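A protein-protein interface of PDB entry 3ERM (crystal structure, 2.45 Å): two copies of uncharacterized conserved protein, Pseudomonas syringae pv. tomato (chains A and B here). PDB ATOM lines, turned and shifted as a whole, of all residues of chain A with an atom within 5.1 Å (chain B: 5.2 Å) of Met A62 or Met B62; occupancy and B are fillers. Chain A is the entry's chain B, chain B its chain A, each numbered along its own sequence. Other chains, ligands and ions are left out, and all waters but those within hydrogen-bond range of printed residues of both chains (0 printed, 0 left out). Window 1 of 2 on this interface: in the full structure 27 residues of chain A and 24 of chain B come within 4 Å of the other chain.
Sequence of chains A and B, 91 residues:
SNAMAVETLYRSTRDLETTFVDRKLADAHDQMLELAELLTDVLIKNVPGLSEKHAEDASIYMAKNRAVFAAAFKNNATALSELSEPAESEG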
ATOM      1  N   LEU A  39      -3.374  23.536 -19.982  1.00  0.00           N
ATOM      2  CA  LEU A  39      -4.644  22.874 -19.934  1.00  0.00           C
ATOM      3  C   LEU A  39      -5.589  23.447 -18.867  1.00  0.00           C
ATOM      4  O   LEU A  39      -6.762  23.719 -19.155  1.00  0.00           O
ATOM      5  CB  LEU A  39      -4.371  21.423 -19.651  1.00  0.00           C
ATOM      6  CG  LEU A  39      -5.208  20.342 -20.298  1.00  0.00           C
ATOM      7  CD1 LEU A  39      -6.206  20.971 -21.260  1.00  0.00           C
ATOM      8  CD2 LEU A  39      -4.264  19.373 -21.002  1.00  0.00           C
ATOM      9  N   LEU A  43      -9.406  25.316 -19.723  1.00  0.00           N
ATOM     10  CA  LEU A  43     -10.603  24.729 -19.096  1.00  0.00           C
ATOM     11  C   LEU A  43     -11.305  25.742 -18.193  1.00  0.00           C
ATOM     12  O   LEU A  43     -12.506  26.000 -18.333  1.00  0.00           O
ATOM     13  CB  LEU A  43     -10.254  23.448 -18.314  1.00  0.00           C
ATOM     14  CG  LEU A  43      -9.735  22.262 -19.168  1.00  0.00           C
ATOM     15  CD1 LEU A  43      -9.312  21.037 -18.265  1.00  0.00           C
ATOM     16  CD2 LEU A  43     -10.691  21.815 -20.265  1.00  0.00           C
ATOM     17  N   ALA A  58      -8.141  17.638 -13.374  1.00  0.00           N
ATOM     18  CA  ALA A  58      -8.502  17.054 -14.641  1.00  0.00           C
ATOM     19  C   ALA A  58      -7.323  17.143 -15.612  1.00  0.00           C
ATOM     20  O   ALA A  58      -6.984  16.155 -16.313  1.00  0.00           O
ATOM     21  CB  ALA A  58      -9.734  17.786 -15.219  1.00  0.00           C
ATOM     22  N   SER A  59      -6.694  18.327 -15.645  1.00  0.00           N
ATOM     23  CA  SER A  59      -5.546  18.579 -16.512  1.00  0.00           C
ATOM     24  C   SER A  59      -4.402  17.672 -16.161  1.00  0.00           C
ATOM     25  O   SER A  59      -3.787  17.082 -17.052  1.00  0.00           O
ATOM     26  CB  SER A  59      -5.103  20.011 -16.364  1.00  0.00           C
ATOM     27  OG  SER A  59      -6.076  20.846 -16.960  1.00  0.00           O
ATOM     28  N   ILE A  60      -4.126  17.531 -14.852  1.00  0.00           N
ATOM     29  CA  ILE A  60      -3.009  16.684 -14.426  1.00  0.00           C
ATOM     30  C   ILE A  60      -3.328  15.263 -14.826  1.00  0.00           C
ATOM     31  O   ILE A  60      -2.492  14.570 -15.386  1.00  0.00           O
ATOM     32  CB  ILE A  60      -2.737  16.789 -12.902  1.00  0.00           C
ATOM     33  CG1 ILE A  60      -1.984  18.070 -12.622  1.00  0.00           C
ATOM     34  CG2 ILE A  60      -1.922  15.599 -12.400  1.00  0.00           C
ATOM     35  CD1 ILE A  60      -1.811  18.286 -11.185  1.00  0.00           C
ATOM     36  N   TYR A  61      -4.567  14.845 -14.616  1.00  0.00           N
ATOM     37  CA  TYR A  61      -4.926  13.483 -15.008  1.00  0.00           C
ATOM     38  C   TYR A  61      -4.698  13.181 -16.511  1.00  0.00           C
ATOM     39  O   TYR A  61      -4.322  12.049 -16.881  1.00  0.00           O
ATOM     40  CB  TYR A  61      -6.388  13.131 -14.636  1.00  0.00           C
ATOM     41  CG  TYR A  61      -6.737  11.741 -15.159  1.00  0.00           C
ATOM     42  CD1 TYR A  61      -6.341  10.587 -14.450  1.00  0.00           C
ATOM     43  CD2 TYR A  61      -7.382  11.574 -16.405  1.00  0.00           C
ATOM     44  CE1 TYR A  61      -6.604   9.306 -14.971  1.00  0.00           C
ATOM     45  CE2 TYR A  61      -7.666  10.308 -16.917  1.00  0.00           C
ATOM     46  CZ  TYR A  61      -7.284   9.192 -16.197  1.00  0.00           C
ATOM     47  OH  TYR A  61      -7.575   7.947 -16.681  1.00  0.00           O
ATOM     48  N   MET A  62      -4.971  14.163 -17.364  1.00  0.00           N
ATOM     49  CA  MET A  62      -4.916  13.931 -18.782  1.00  0.00           C
ATOM     50  C   MET A  62      -3.472  14.058 -19.197  1.00  0.00           C
ATOM     51  O   MET A  62      -2.983  13.254 -20.012  1.00  0.00           O
ATOM     52  CB  MET A  62      -5.762  14.967 -19.555  1.00  0.00           C
ATOM     53  CG  MET A  62      -7.268  14.822 -19.310  1.00  0.00           C
ATOM     54  SD  MET A  62      -8.289  15.944 -20.537  1.00  0.00           S
ATOM     55  CE  MET A  62      -8.491  17.472 -19.362  1.00  0.00           C
ATOM     56  N   ALA A  63      -2.781  15.075 -18.656  1.00  0.00           N
ATOM     57  CA  ALA A  63      -1.399  15.367 -19.061  1.00  0.00           C
ATOM     58  C   ALA A  63      -0.489  14.201 -18.663  1.00  0.00           C
ATOM     59  O   ALA A  63       0.450  13.837 -19.359  1.00  0.00           O
ATOM     60  CB  ALA A  63      -0.909  16.672 -18.403  1.00  0.00           C
ATOM     61  N   LYS A  64      -0.794  13.651 -17.501  1.00  0.00           N
ATOM     62  CA  LYS A  64      -0.152  12.483 -16.941  1.00  0.00           C
ATOM     63  C   LYS A  64      -0.344  11.274 -17.868  1.00  0.00           C
ATOM     64  O   LYS A  64       0.423  10.284 -17.826  1.00  0.00           O
ATOM     65  CB  LYS A  64      -0.896  12.216 -15.659  1.00  0.00           C
ATOM     66  CG  LYS A  64      -0.310  11.247 -14.848  1.00  0.00           C
ATOM     67  CD  LYS A  64      -0.984  11.301 -13.495  1.00  0.00           C
ATOM     68  CE  LYS A  64      -2.324  10.700 -13.638  1.00  0.00           C
ATOM     69  NZ  LYS A  64      -2.547  10.027 -12.352  1.00  0.00           N
ATOM     70  N   ASN A  65      -1.408  11.339 -18.674  1.00  0.00           N
ATOM     71  CA  ASN A  65      -1.779  10.225 -19.540  1.00  0.00           C
ATOM     72  C   ASN A  65      -1.700  10.638 -21.000  1.00  0.00           C
ATOM     73  O   ASN A  65      -2.497  10.182 -21.820  1.00  0.00           O
ATOM     74  CB  ASN A  65      -3.196   9.758 -19.181  1.00  0.00           C
ATOM     75  CG  ASN A  65      -3.230   8.897 -17.934  1.00  0.00           C
ATOM     76  OD1 ASN A  65      -2.774   7.751 -17.964  1.00  0.00           O
ATOM     77  ND2 ASN A  65      -3.775   9.438 -16.834  1.00  0.00           N
ATOM     78  N   ARG A  66      -0.737  11.499 -21.313  1.00  0.00           N
ATOM     79  CA  ARG A  66      -0.825  12.256 -22.556  1.00  0.00           C
ATOM     80  C   ARG A  66      -0.830  11.424 -23.811  1.00  0.00           C
ATOM     81  O   ARG A  66      -1.574  11.761 -24.728  1.00  0.00           O
ATOM     82  CB  ARG A  66       0.174  13.426 -22.651  1.00  0.00           C
ATOM     83  CG  ARG A  66       1.625  13.070 -22.818  1.00  0.00           C
ATOM     84  CD  ARG A  66       2.502  14.336 -22.839  1.00  0.00           C
ATOM     85  NE  ARG A  66       2.085  15.336 -23.846  1.00  0.00           N
ATOM     86  CZ  ARG A  66       2.831  16.369 -24.280  1.00  0.00           C
ATOM     87  NH1 ARG A  66       4.062  16.571 -23.847  1.00  0.00           N
ATOM     88  NH2 ARG A  66       2.355  17.218 -25.166  1.00  0.00           N
ATOM     89  N   PHE A  69      -4.244  10.007 -24.442  1.00  0.00           N
ATOM     90  CA  PHE A  69      -5.151  11.078 -24.911  1.00  0.00           C
ATOM     91  C   PHE A  69      -4.818  11.566 -26.324  1.00  0.00           C
ATOM     92  O   PHE A  69      -5.734  11.783 -27.140  1.00  0.00           O
ATOM     93  CB  PHE A  69      -5.254  12.252 -23.931  1.00  0.00           C
ATOM     94  CG  PHE A  69      -6.075  11.937 -22.706  1.00  0.00           C
ATOM     95  CD1 PHE A  69      -5.524  11.257 -21.635  1.00  0.00           C
ATOM     96  CD2 PHE A  69      -7.426  12.301 -22.641  1.00  0.00           C
ATOM     97  CE1 PHE A  69      -6.292  10.939 -20.505  1.00  0.00           C
ATOM     98  CE2 PHE A  69      -8.204  11.997 -21.513  1.00  0.00           C
ATOM     99  CZ  PHE A  69      -7.627  11.307 -20.440  1.00  0.00           C
ATOM    100  N   PHE A  73      -7.437  11.703 -29.292  1.00  0.00           N
ATOM    101  CA  PHE A  73      -7.813  12.937 -29.966  1.00  0.00           C
ATOM    102  C   PHE A  73      -7.504  12.868 -31.440  1.00  0.00           C
ATOM    103  O   PHE A  73      -8.298  13.317 -32.231  1.00  0.00           O
ATOM    104  CB  PHE A  73      -7.082  14.141 -29.378  1.00  0.00           C
ATOM    105  CG  PHE A  73      -7.702  14.681 -28.142  1.00  0.00           C
ATOM    106  CD1 PHE A  73      -8.975  15.235 -28.173  1.00  0.00           C
ATOM    107  CD2 PHE A  73      -7.002  14.676 -26.937  1.00  0.00           C
ATOM    108  CE1 PHE A  73      -9.558  15.746 -27.005  1.00  0.00           C
ATOM    109  CE2 PHE A  73      -7.586  15.208 -25.749  1.00  0.00           C
ATOM    110  CZ  PHE A  73      -8.869  15.721 -25.802  1.00  0.00           C
ATOM    111  N   LEU B  39     -14.841  10.650 -23.362  1.00  0.00           N
ATOM    112  CA  LEU B  39     -14.109  11.574 -22.481  1.00  0.00           C
ATOM    113  C   LEU B  39     -14.828  11.913 -21.171  1.00  0.00           C
ATOM    114  O   LEU B  39     -14.198  11.982 -20.108  1.00  0.00           O
ATOM    115  CB  LEU B  39     -13.866  12.882 -23.202  1.00  0.00           C
ATOM    116  CG  LEU B  39     -12.509  13.438 -23.644  1.00  0.00           C
ATOM    117  CD1 LEU B  39     -11.341  12.463 -23.609  1.00  0.00           C
ATOM    118  CD2 LEU B  39     -12.715  14.072 -25.043  1.00  0.00           C
ATOM    119  N   LEU B  43     -13.424  10.952 -17.465  1.00  0.00           N
ATOM    120  CA  LEU B  43     -13.221  12.036 -16.529  1.00  0.00           C
ATOM    121  C   LEU B  43     -14.005  11.864 -15.249  1.00  0.00           C
ATOM    122  O   LEU B  43     -13.440  12.019 -14.149  1.00  0.00           O
ATOM    123  CB  LEU B  43     -13.520  13.385 -17.161  1.00  0.00           C
ATOM    124  CG  LEU B  43     -12.515  13.876 -18.219  1.00  0.00           C
ATOM    125  CD1 LEU B  43     -12.999  15.253 -18.736  1.00  0.00           C
ATOM    126  CD2 LEU B  43     -11.092  13.983 -17.658  1.00  0.00           C
ATOM    127  N   ALA B  58     -16.642  20.102 -20.581  1.00  0.00           N
ATOM    128  CA  ALA B  58     -15.239  20.179 -20.911  1.00  0.00           C
ATOM    129  C   ALA B  58     -14.930  19.172 -22.009  1.00  0.00           C
ATOM    130  O   ALA B  58     -14.091  19.425 -22.860  1.00  0.00           O
ATOM    131  CB  ALA B  58     -14.409  19.901 -19.673  1.00  0.00           C
ATOM    132  N   SER B  59     -15.630  18.038 -21.974  1.00  0.00           N
ATOM    133  CA  SER B  59     -15.477  16.971 -22.966  1.00  0.00           C
ATOM    134  C   SER B  59     -15.942  17.418 -24.335  1.00  0.00           C
ATOM    135  O   SER B  59     -15.265  17.128 -25.321  1.00  0.00           O
ATOM    136  CB  SER B  59     -16.273  15.732 -22.557  1.00  0.00           C
ATOM    137  OG  SER B  59     -15.589  15.102 -21.504  1.00  0.00           O
ATOM    138  N   ILE B  60     -17.088  18.113 -24.387  1.00  0.00           N
ATOM    139  CA  ILE B  60     -17.629  18.629 -25.643  1.00  0.00           C
ATOM    140  C   ILE B  60     -16.665  19.657 -26.177  1.00  0.00           C
ATOM    141  O   ILE B  60     -16.480  19.782 -27.370  1.00  0.00           O
ATOM    142  CB  ILE B  60     -19.007  19.283 -25.458  1.00  0.00           C
ATOM    143  CG1 ILE B  60     -20.038  18.243 -25.017  1.00  0.00           C
ATOM    144  CG2 ILE B  60     -19.507  19.942 -26.765  1.00  0.00           C
ATOM    145  CD1 ILE B  60     -21.480  18.762 -24.995  1.00  0.00           C
ATOM    146  N   TYR B  61     -16.013  20.379 -25.289  1.00  0.00           N
ATOM    147  CA  TYR B  61     -15.220  21.498 -25.726  1.00  0.00           C
ATOM    148  C   TYR B  61     -13.955  20.993 -26.401  1.00  0.00           C
ATOM    149  O   TYR B  61     -13.581  21.447 -27.487  1.00  0.00           O
ATOM    150  CB  TYR B  61     -14.866  22.403 -24.553  1.00  0.00           C
ATOM    151  CG  TYR B  61     -13.827  23.418 -24.914  1.00  0.00           C
ATOM    152  CD1 TYR B  61     -14.163  24.529 -25.716  1.00  0.00           C
ATOM    153  CD2 TYR B  61     -12.490  23.246 -24.532  1.00  0.00           C
ATOM    154  CE1 TYR B  61     -13.189  25.485 -26.090  1.00  0.00           C
ATOM    155  CE2 TYR B  61     -11.494  24.189 -24.902  1.00  0.00           C
ATOM    156  CZ  TYR B  61     -11.854  25.310 -25.664  1.00  0.00           C
ATOM    157  OH  TYR B  61     -10.906  26.262 -26.024  1.00  0.00           O
ATOM    158  N   MET B  62     -13.302  20.062 -25.725  1.00  0.00           N
ATOM    159  CA  MET B  62     -12.130  19.376 -26.254  1.00  0.00           C
ATOM    160  C   MET B  62     -12.481  18.648 -27.553  1.00  0.00           C
ATOM    161  O   MET B  62     -11.747  18.771 -28.526  1.00  0.00           O
ATOM    162  CB  MET B  62     -11.559  18.388 -25.220  1.00  0.00           C
ATOM    163  CG  MET B  62     -11.411  18.993 -23.843  1.00  0.00           C
ATOM    164  SD  MET B  62     -10.182  17.973 -22.697  1.00  0.00           S
ATOM    165  CE  MET B  62      -8.739  19.129 -22.751  1.00  0.00           C
ATOM    166  N   ALA B  63     -13.591  17.893 -27.551  1.00  0.00           N
ATOM    167  CA  ALA B  63     -13.977  17.125 -28.718  1.00  0.00           C
ATOM    168  C   ALA B  63     -14.138  18.079 -29.907  1.00  0.00           C
ATOM    169  O   ALA B  63     -13.613  17.797 -30.961  1.00  0.00           O
ATOM    170  CB  ALA B  63     -15.248  16.310 -28.469  1.00  0.00           C
ATOM    171  N   LYS B  64     -14.785  19.236 -29.721  1.00  0.00           N
ATOM    172  CA  LYS B  64     -14.930  20.244 -30.807  1.00  0.00           C
ATOM    173  C   LYS B  64     -13.587  20.855 -31.270  1.00  0.00           C
ATOM    174  O   LYS B  64     -13.527  21.512 -32.300  1.00  0.00           O
ATOM    175  CB  LYS B  64     -15.839  21.389 -30.376  1.00  0.00           C
ATOM    176  CG  LYS B  64     -17.355  21.124 -30.310  1.00  0.00           C
ATOM    177  CD  LYS B  64     -18.051  22.361 -29.660  1.00  0.00           C
ATOM    178  CE  LYS B  64     -19.570  22.235 -29.434  1.00  0.00           C
ATOM    179  NZ  LYS B  64     -20.413  22.698 -30.582  1.00  0.00           N
ATOM    180  N   ASN B  65     -12.521  20.680 -30.487  1.00  0.00           N
ATOM    181  CA  ASN B  65     -11.212  21.201 -30.844  1.00  0.00           C
ATOM    182  C   ASN B  65     -10.209  20.078 -30.835  1.00  0.00           C
ATOM    183  O   ASN B  65      -9.032  20.263 -30.424  1.00  0.00           O
ATOM    184  CB  ASN B  65     -10.830  22.210 -29.813  1.00  0.00           C
ATOM    185  CG  ASN B  65     -11.788  23.353 -29.789  1.00  0.00           C
ATOM    186  OD1 ASN B  65     -11.705  24.233 -30.605  1.00  0.00           O
ATOM    187  ND2 ASN B  65     -12.724  23.336 -28.857  1.00  0.00           N
ATOM    188  N   ARG B  66     -10.682  18.891 -31.249  1.00  0.00           N
ATOM    189  CA  ARG B  66      -9.854  17.696 -31.102  1.00  0.00           C
ATOM    190  C   ARG B  66      -8.512  17.794 -31.816  1.00  0.00           C
ATOM    191  O   ARG B  66      -7.522  17.235 -31.313  1.00  0.00           O
ATOM    192  CB  ARG B  66     -10.590  16.382 -31.440  1.00  0.00           C
ATOM    193  CG  ARG B  66     -10.974  16.206 -32.848  1.00  0.00           C
ATOM    194  CD  ARG B  66     -11.789  14.928 -33.035  1.00  0.00           C
ATOM    195  NE  ARG B  66     -11.043  13.692 -32.725  1.00  0.00           N
ATOM    196  CZ  ARG B  66     -11.569  12.460 -32.733  1.00  0.00           C
ATOM    197  NH1 ARG B  66     -12.847  12.257 -33.049  1.00  0.00           N
ATOM    198  NH2 ARG B  66     -10.810  11.419 -32.428  1.00  0.00           N
ATOM    199  N   PHE B  69      -6.179  19.863 -29.612  1.00  0.00           N
ATOM    200  CA  PHE B  69      -5.799  19.063 -28.441  1.00  0.00           C
ATOM    201  C   PHE B  69      -4.857  17.913 -28.818  1.00  0.00           C
ATOM    202  O   PHE B  69      -3.854  17.694 -28.132  1.00  0.00           O
ATOM    203  CB  PHE B  69      -7.023  18.623 -27.637  1.00  0.00           C
ATOM    204  CG  PHE B  69      -7.629  19.755 -26.793  1.00  0.00           C
ATOM    205  CD1 PHE B  69      -8.578  20.616 -27.328  1.00  0.00           C
ATOM    206  CD2 PHE B  69      -7.230  19.962 -25.480  1.00  0.00           C
ATOM    207  CE1 PHE B  69      -9.109  21.662 -26.568  1.00  0.00           C
ATOM    208  CE2 PHE B  69      -7.771  21.010 -24.696  1.00  0.00           C
ATOM    209  CZ  PHE B  69      -8.711  21.851 -25.240  1.00  0.00           C
ATOM    210  N   PHE B  73      -1.259  17.477 -26.986  1.00  0.00           N
ATOM    211  CA  PHE B  73      -0.873  16.237 -26.330  1.00  0.00           C
ATOM    212  C   PHE B  73       0.230  15.481 -27.059  1.00  0.00           C
ATOM    213  O   PHE B  73       1.095  14.916 -26.400  1.00  0.00           O
ATOM    214  CB  PHE B  73      -2.089  15.314 -26.155  1.00  0.00           C
ATOM    215  CG  PHE B  73      -2.967  15.681 -24.998  1.00  0.00           C
ATOM    216  CD1 PHE B  73      -2.867  15.008 -23.803  1.00  0.00           C
ATOM    217  CD2 PHE B  73      -3.910  16.695 -25.104  1.00  0.00           C
ATOM    218  CE1 PHE B  73      -3.680  15.328 -22.737  1.00  0.00           C
ATOM    219  CE2 PHE B  73      -4.744  17.019 -24.029  1.00  0.00           C
ATOM    220  CZ  PHE B  73      -4.615  16.339 -22.849  1.00  0.00           C
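Among the printed residues, merely in contact across the chains: Leu A39 with Met B62 (3.5 Å), Leu A39 with Phe B69 (3.8 Å), Leu A39 with Phe B73 (3.6 Å), Met A62 with Phe B73 (3.5 Å), Phe A69 with Leu B39 (3.8 Å), Phe A69 with Phe B73 (3.6 Å), Phe A73 with Met B62 (3.8 Å), Phe A73 with Phe B69 (3.9 Å) and Phe A73 with Phe B73 (3.8 Å).
Of the 13 printed residues of chain B, 5 touch a printed residue of chain A.
Hydrophobic or aromatic side chains of chain B within 4 Å of the printed part of chain A: Leu B39, Met B62, Phe B69 and Phe B73.
Of the 13 printed residues of chain A, 5 touch a printed residue of chain B.
Leu A39 touches Met B62, but with the chains exchanged Met A62 does not touch Leu B39 (5.6 Å).
Met A62 touches its own counterpart, Met B62.
Met A62 touches Phe B73, and with the chains exchanged Phe A73 touches Met B62.
Arg A66 touches Phe B73, and with the chains exchanged Phe A73 touches Arg B66.
13 positions are printed for both chains.
Of the printed residues of chain B, Leu A39 touches Met B62 (3.5 Å), Phe B69 (3.8 Å) and Phe B73 (3.6 Å).
Met A62 touches two residues of chain B.
Of the printed residues of chain B, Arg A66 touches Phe B73.
Of the printed residues of chain B, Phe A69 touches Leu B39 and Phe B73.
Ser B59 touches none of the printed residues of chain A.
Of the printed residues of chain A, Phe B73 touches Leu A39, Met A62, Arg A66, Phe A69 and Phe A73.
The nearest residue of chain B that does not touch Met A62 is Leu B43 (4.2 Å).
The nearest printed residue of chain A that does not touch Arg B66 is Phe A69 (7.1 Å).
The guanidinium group of Arg B66 sits at hydrogen-bond distance from the backbone carbonyl oxygen of Phe A73 (2.8 Å).
The side-chain sulfur of Met A62 lies close to the side-chain sulfur of Met B62 (3.5 Å).
NE of Arg A66 sits at hydrogen-bond distance from O of Phe B73, 2.8 Å away.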
